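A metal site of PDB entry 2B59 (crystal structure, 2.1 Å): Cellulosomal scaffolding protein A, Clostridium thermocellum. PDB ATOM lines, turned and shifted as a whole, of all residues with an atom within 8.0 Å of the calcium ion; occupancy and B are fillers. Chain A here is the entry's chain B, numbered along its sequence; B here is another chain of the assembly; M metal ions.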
ATOM      1  N   VAL A 117     -17.990 -25.692 -12.025  1.00  0.00           N
ATOM      2  CA  VAL A 117     -18.835 -24.565 -11.664  1.00  0.00           C
ATOM      3  C   VAL A 117     -18.526 -24.180 -10.221  1.00  0.00           C
ATOM      4  O   VAL A 117     -18.475 -22.986  -9.886  1.00  0.00           O
ATOM      5  CB  VAL A 117     -20.334 -24.928 -11.777  1.00  0.00           C
ATOM      6  CG1 VAL A 117     -21.191 -23.725 -11.389  1.00  0.00           C
ATOM      7  CG2 VAL A 117     -20.660 -25.377 -13.188  1.00  0.00           C
ATOM      8  N   ALA A 123     -19.027 -16.340  -7.677  1.00  0.00           N
ATOM      9  CA  ALA A 123     -18.369 -15.296  -8.455  1.00  0.00           C
ATOM     10  C   ALA A 123     -19.439 -14.414  -9.104  1.00  0.00           C
ATOM     11  O   ALA A 123     -20.492 -14.903  -9.506  1.00  0.00           O
ATOM     12  CB  ALA A 123     -17.481 -15.917  -9.530  1.00  0.00           C
ATOM     13  N   TYR A 130     -14.945 -14.901 -12.131  1.00  0.00           N
ATOM     14  CA  TYR A 130     -16.147 -15.056 -12.941  1.00  0.00           C
ATOM     15  C   TYR A 130     -15.833 -15.433 -14.392  1.00  0.00           C
ATOM     16  O   TYR A 130     -14.984 -14.811 -15.032  1.00  0.00           O
ATOM     17  CB  TYR A 130     -16.978 -13.771 -12.905  1.00  0.00           C
ATOM     18  CG  TYR A 130     -18.249 -13.836 -13.727  1.00  0.00           C
ATOM     19  CD1 TYR A 130     -18.234 -13.536 -15.089  1.00  0.00           C
ATOM     20  CD2 TYR A 130     -19.472 -14.164 -13.129  1.00  0.00           C
ATOM     21  CE1 TYR A 130     -19.401 -13.584 -15.853  1.00  0.00           C
ATOM     22  CE2 TYR A 130     -20.646 -14.216 -13.878  1.00  0.00           C
ATOM     23  CZ  TYR A 130     -20.611 -13.926 -15.240  1.00  0.00           C
ATOM     24  OH  TYR A 130     -21.762 -13.954 -15.983  1.00  0.00           O
ATOM     25  N   GLU A 132     -18.104 -16.184 -17.784  1.00  0.00           N
ATOM     26  CA  GLU A 132     -19.442 -16.157 -18.354  1.00  0.00           C
ATOM     27  C   GLU A 132     -20.023 -17.531 -18.739  1.00  0.00           C
ATOM     28  O   GLU A 132     -21.189 -17.804 -18.431  1.00  0.00           O
ATOM     29  CB  GLU A 132     -19.499 -15.211 -19.564  1.00  0.00           C
ATOM     30  CG  GLU A 132     -20.921 -14.886 -20.009  1.00  0.00           C
ATOM     31  CD  GLU A 132     -20.972 -13.792 -21.073  1.00  0.00           C
ATOM     32  OE1 GLU A 132     -22.093 -13.309 -21.374  1.00  0.00           O
ATOM     33  OE2 GLU A 132     -19.907 -13.409 -21.604  1.00  0.00           O
ATOM     34  N   LEU A 134     -19.638 -20.319 -17.450  1.00  0.00           N
ATOM     35  CA  LEU A 134     -20.009 -21.099 -16.271  1.00  0.00           C
ATOM     36  C   LEU A 134     -21.231 -20.498 -15.580  1.00  0.00           C
ATOM     37  O   LEU A 134     -21.841 -21.124 -14.713  1.00  0.00           O
ATOM     38  CB  LEU A 134     -18.819 -21.194 -15.307  1.00  0.00           C
ATOM     39  CG  LEU A 134     -17.574 -21.859 -15.921  1.00  0.00           C
ATOM     40  CD1 LEU A 134     -16.470 -21.927 -14.883  1.00  0.00           C
ATOM     41  CD2 LEU A 134     -17.925 -23.253 -16.426  1.00  0.00           C
ATOM     42  N   ASP A 135     -21.580 -19.278 -15.977  1.00  0.00           N
ATOM     43  CA  ASP A 135     -22.760 -18.603 -15.449  1.00  0.00           C
ATOM     44  C   ASP A 135     -23.894 -19.089 -16.355  1.00  0.00           C
ATOM     45  O   ASP A 135     -24.388 -18.345 -17.206  1.00  0.00           O
ATOM     46  CB  ASP A 135     -22.578 -17.082 -15.559  1.00  0.00           C
ATOM     47  CG  ASP A 135     -23.836 -16.321 -15.183  1.00  0.00           C
ATOM     48  OD1 ASP A 135     -24.818 -16.974 -14.788  1.00  0.00           O
ATOM     49  OD2 ASP A 135     -23.850 -15.076 -15.288  1.00  0.00           O
ATOM     50  N   ILE A 136     -24.283 -20.347 -16.167  1.00  0.00           N
ATOM     51  CA  ILE A 136     -25.319 -21.025 -16.947  1.00  0.00           C
ATOM     52  C   ILE A 136     -26.528 -20.222 -17.409  1.00  0.00           C
ATOM     53  O   ILE A 136     -26.808 -20.189 -18.603  1.00  0.00           O
ATOM     54  CB  ILE A 136     -25.833 -22.291 -16.217  1.00  0.00           C
ATOM     55  CG1 ILE A 136     -24.650 -23.154 -15.768  1.00  0.00           C
ATOM     56  CG2 ILE A 136     -26.733 -23.103 -17.148  1.00  0.00           C
ATOM     57  CD1 ILE A 136     -23.823 -23.727 -16.905  1.00  0.00           C
ATOM     58  N   ASN A 137     -27.264 -19.597 -16.492  1.00  0.00           N
ATOM     59  CA  ASN A 137     -28.434 -18.835 -16.901  1.00  0.00           C
ATOM     60  C   ASN A 137     -28.107 -17.361 -17.190  1.00  0.00           C
ATOM     61  O   ASN A 137     -29.007 -16.553 -17.434  1.00  0.00           O
ATOM     62  CB  ASN A 137     -29.567 -18.952 -15.858  1.00  0.00           C
ATOM     63  CG  ASN A 137     -29.228 -18.288 -14.529  1.00  0.00           C
ATOM     64  OD1 ASN A 137     -28.148 -17.774 -14.355  1.00  0.00           O
ATOM     65  ND2 ASN A 137     -30.186 -18.305 -13.601  1.00  0.00           N
ATOM     66  N   ARG A 138     -26.817 -17.035 -17.148  1.00  0.00           N
ATOM     67  CA  ARG A 138     -26.336 -15.681 -17.453  1.00  0.00           C
ATOM     68  C   ARG A 138     -26.979 -14.537 -16.655  1.00  0.00           C
ATOM     69  O   ARG A 138     -27.171 -13.448 -17.198  1.00  0.00           O
ATOM     70  CB  ARG A 138     -26.540 -15.387 -18.941  1.00  0.00           C
ATOM     71  CG  ARG A 138     -25.934 -16.406 -19.906  1.00  0.00           C
ATOM     72  CD  ARG A 138     -24.446 -16.171 -20.124  1.00  0.00           C
ATOM     73  NE  ARG A 138     -24.041 -16.536 -21.478  1.00  0.00           N
ATOM     74  CZ  ARG A 138     -23.780 -17.775 -21.874  1.00  0.00           C
ATOM     75  NH1 ARG A 138     -23.875 -18.769 -20.998  1.00  0.00           N
ATOM     76  NH2 ARG A 138     -23.442 -18.026 -23.128  1.00  0.00           N
ATOM     77  N   ASN A 139     -27.307 -14.768 -15.386  1.00  0.00           N
ATOM     78  CA  ASN A 139     -27.934 -13.702 -14.592  1.00  0.00           C
ATOM     79  C   ASN A 139     -26.924 -12.837 -13.830  1.00  0.00           C
ATOM     80  O   ASN A 139     -27.312 -12.001 -13.013  1.00  0.00           O
ATOM     81  CB  ASN A 139     -28.970 -14.278 -13.619  1.00  0.00           C
ATOM     82  CG  ASN A 139     -28.345 -15.072 -12.510  1.00  0.00           C
ATOM     83  OD1 ASN A 139     -27.137 -15.291 -12.496  1.00  0.00           O
ATOM     84  ND2 ASN A 139     -29.163 -15.525 -11.549  1.00  0.00           N
ATOM     85  N   GLY A 140     -25.629 -13.031 -14.100  1.00  0.00           N
ATOM     86  CA  GLY A 140     -24.613 -12.223 -13.449  1.00  0.00           C
ATOM     87  C   GLY A 140     -23.878 -12.813 -12.252  1.00  0.00           C
ATOM     88  O   GLY A 140     -23.008 -12.153 -11.682  1.00  0.00           O
ATOM     89  N   ALA A 141     -24.215 -14.042 -11.866  1.00  0.00           N
ATOM     90  CA  ALA A 141     -23.546 -14.669 -10.727  1.00  0.00           C
ATOM     91  C   ALA A 141     -23.491 -16.169 -10.922  1.00  0.00           C
ATOM     92  O   ALA A 141     -24.365 -16.736 -11.529  1.00  0.00           O
ATOM     93  CB  ALA A 141     -24.282 -14.334  -9.442  1.00  0.00           C
ATOM     94  N   ILE A 142     -22.456 -16.812 -10.400  1.00  0.00           N
ATOM     95  CA  ILE A 142     -22.332 -18.263 -10.510  1.00  0.00           C
ATOM     96  C   ILE A 142     -22.673 -18.818  -9.133  1.00  0.00           C
ATOM     97  O   ILE A 142     -21.983 -18.517  -8.161  1.00  0.00           O
ATOM     98  CB  ILE A 142     -20.902 -18.663 -10.922  1.00  0.00           C
ATOM     99  CG1 ILE A 142     -20.582 -18.101 -12.307  1.00  0.00           C
ATOM    100  CG2 ILE A 142     -20.765 -20.189 -10.902  1.00  0.00           C
ATOM    101  CD1 ILE A 142     -19.144 -18.337 -12.768  1.00  0.00           C
ATOM    102  N   ASN A 143     -23.726 -19.618  -9.059  1.00  0.00           N
ATOM    103  CA  ASN A 143     -24.156 -20.159  -7.770  1.00  0.00           C
ATOM    104  C   ASN A 143     -24.922 -21.476  -7.872  1.00  0.00           C
ATOM    105  O   ASN A 143     -24.897 -22.148  -8.911  1.00  0.00           O
ATOM    106  CB  ASN A 143     -25.026 -19.104  -7.061  1.00  0.00           C
ATOM    107  CG  ASN A 143     -26.149 -18.582  -7.944  1.00  0.00           C
ATOM    108  OD1 ASN A 143     -26.720 -19.332  -8.729  1.00  0.00           O
ATOM    109  ND2 ASN A 143     -26.461 -17.292  -7.813  1.00  0.00           N
ATOM    110  N   MET A 144     -25.621 -21.845  -6.795  1.00  0.00           N
ATOM    111  CA  MET A 144     -26.369 -23.099  -6.773  1.00  0.00           C
ATOM    112  C   MET A 144     -27.459 -23.200  -7.853  1.00  0.00           C
ATOM    113  O   MET A 144     -27.785 -24.299  -8.301  1.00  0.00           O
ATOM    114  CB  MET A 144     -26.971 -23.339  -5.396  1.00  0.00           C
ATOM    115  CG  MET A 144     -27.687 -24.689  -5.240  1.00  0.00           C
ATOM    116  SD  MET A 144     -26.627 -26.143  -5.521  1.00  0.00           S
ATOM    117  CE  MET A 144     -27.300 -26.773  -6.946  1.00  0.00           C
ATOM    118  N   GLN A 145     -28.026 -22.062  -8.245  1.00  0.00           N
ATOM    119  CA  GLN A 145     -29.071 -22.074  -9.272  1.00  0.00           C
ATOM    120  C   GLN A 145     -28.516 -22.666 -10.585  1.00  0.00           C
ATOM    121  O   GLN A 145     -29.211 -23.396 -11.286  1.00  0.00           O
ATOM    122  CB  GLN A 145     -29.584 -20.643  -9.513  1.00  0.00           C
ATOM    123  CG  GLN A 145     -30.487 -20.504 -10.736  1.00  0.00           C
ATOM    124  CD  GLN A 145     -31.159 -19.140 -10.835  1.00  0.00           C
ATOM    125  OE1 GLN A 145     -30.549 -18.121 -10.527  1.00  0.00           O
ATOM    126  NE2 GLN A 145     -32.403 -19.125 -11.287  1.00  0.00           N
ATOM    127  N   ASP A 146     -27.267 -22.330 -10.905  1.00  0.00           N
ATOM    128  CA  ASP A 146     -26.636 -22.833 -12.116  1.00  0.00           C
ATOM    129  C   ASP A 146     -26.334 -24.321 -11.994  1.00  0.00           C
ATOM    130  O   ASP A 146     -26.480 -25.073 -12.951  1.00  0.00           O
ATOM    131  CB  ASP A 146     -25.328 -22.104 -12.383  1.00  0.00           C
ATOM    132  CG  ASP A 146     -25.526 -20.635 -12.587  1.00  0.00           C
ATOM    133  OD1 ASP A 146     -25.006 -19.849 -11.761  1.00  0.00           O
ATOM    134  OD2 ASP A 146     -26.216 -20.277 -13.563  1.00  0.00           O
ATOM    135  N   ILE A 147     -25.888 -24.710 -10.808  1.00  0.00           N
ATOM    136  CA  ILE A 147     -25.575 -26.108 -10.549  1.00  0.00           C
ATOM    137  C   ILE A 147     -26.837 -26.950 -10.688  1.00  0.00           C
ATOM    138  O   ILE A 147     -26.810 -28.025 -11.268  1.00  0.00           O
ATOM    139  CB  ILE A 147     -24.960 -26.264  -9.132  1.00  0.00           C
ATOM    140  CG1 ILE A 147     -23.612 -25.537  -9.096  1.00  0.00           C
ATOM    141  CG2 ILE A 147     -24.786 -27.730  -8.791  1.00  0.00           C
ATOM    142  CD1 ILE A 147     -22.958 -25.508  -7.734  1.00  0.00           C
ATOM    143  N   ILE A 149     -29.280 -26.516 -12.627  1.00  0.00           N
ATOM    144  CA  ILE A 149     -29.603 -26.664 -14.045  1.00  0.00           C
ATOM    145  C   ILE A 149     -28.790 -27.832 -14.605  1.00  0.00           C
ATOM    146  O   ILE A 149     -29.307 -28.664 -15.357  1.00  0.00           O
ATOM    147  CB  ILE A 149     -29.285 -25.370 -14.843  1.00  0.00           C
ATOM    148  CG1 ILE A 149     -30.291 -24.284 -14.462  1.00  0.00           C
ATOM    149  CG2 ILE A 149     -29.314 -25.651 -16.347  1.00  0.00           C
ATOM    150  CD1 ILE A 149     -29.963 -22.905 -15.032  1.00  0.00           C
ATOM    151  N   SER B 151     -24.120 -12.127  -4.838  1.00  0.00           N
ATOM    152  CA  SER B 151     -23.839 -13.412  -5.474  1.00  0.00           C
ATOM    153  C   SER B 151     -25.082 -14.296  -5.611  1.00  0.00           C
ATOM    154  O   SER B 151     -25.008 -15.419  -6.103  1.00  0.00           O
ATOM    155  CB  SER B 151     -22.740 -14.159  -4.712  1.00  0.00           C
ATOM    156  OG  SER B 151     -23.199 -14.570  -3.449  1.00  0.00           O
ATOM    157  N   PRO B 153     -28.509 -13.149  -7.026  1.00  0.00           N
ATOM    158  CA  PRO B 153     -29.554 -12.286  -7.594  1.00  0.00           C
ATOM    159  C   PRO B 153     -30.896 -13.001  -7.759  1.00  0.00           C
ATOM    160  O   PRO B 153     -30.948 -14.164  -8.151  1.00  0.00           O
ATOM    161  CB  PRO B 153     -28.935 -11.857  -8.934  1.00  0.00           C
ATOM    162  CG  PRO B 153     -28.050 -13.014  -9.292  1.00  0.00           C
ATOM    163  CD  PRO B 153     -27.404 -13.363  -7.978  1.00  0.00           C
HETATM  164 CA    CA M   1     -26.221 -17.730 -12.759  1.00  0.00          CA
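The backbone NH (N) of Arg 138 sits close to the side-chain carboxylate (OD1) of Asp 135, at 3.1 Å.
The side-chain carboxylate (OD2) of Asp 135 is in hydrogen-bond range of the side-chain hydroxyl (OH) of Tyr 130 (2.5 Å).
The side-chain amide nitrogen of Asn 139 sits at hydrogen-bond distance from the side-chain amide oxygen of Gln 145 (3.1 Å).
OD2 of Asp 135 lies within hydrogen-bond range of N of Gly 140, at 3.0 Å.
The side-chain amide oxygen of Gln 145 lies close to the side-chain amide nitrogen of Asn 137, 3.1 Å away.
The backbone NH (N) of Ile 136 sits close to the side-chain carboxylate (OD2) of Asp 146 (3.2 Å).
N of Asn 143 lies close to OD1 of Asp 146 (3.0 Å).
Five residues have an atom within 4 Å of the calcium ion: Asp 135, Asn 137, Asn 139, Ala 141 and Asp 146.
The nearest printed residue that does not touch the calcium ion is Asn 143 (4.4 Å).
The calcium ion is bound by O of Ala 141 (2.4 Å), OD1 of Asn 137 (2.5 Å), OD1 of Asp 135 (2.6 Å), OD1 of Asn 139 (2.6 Å), OD1 of Asp 146 (2.6 Å) and OD2 of Asp 146 (2.7 Å).
The calcium ion has six donor atoms within binding distance.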
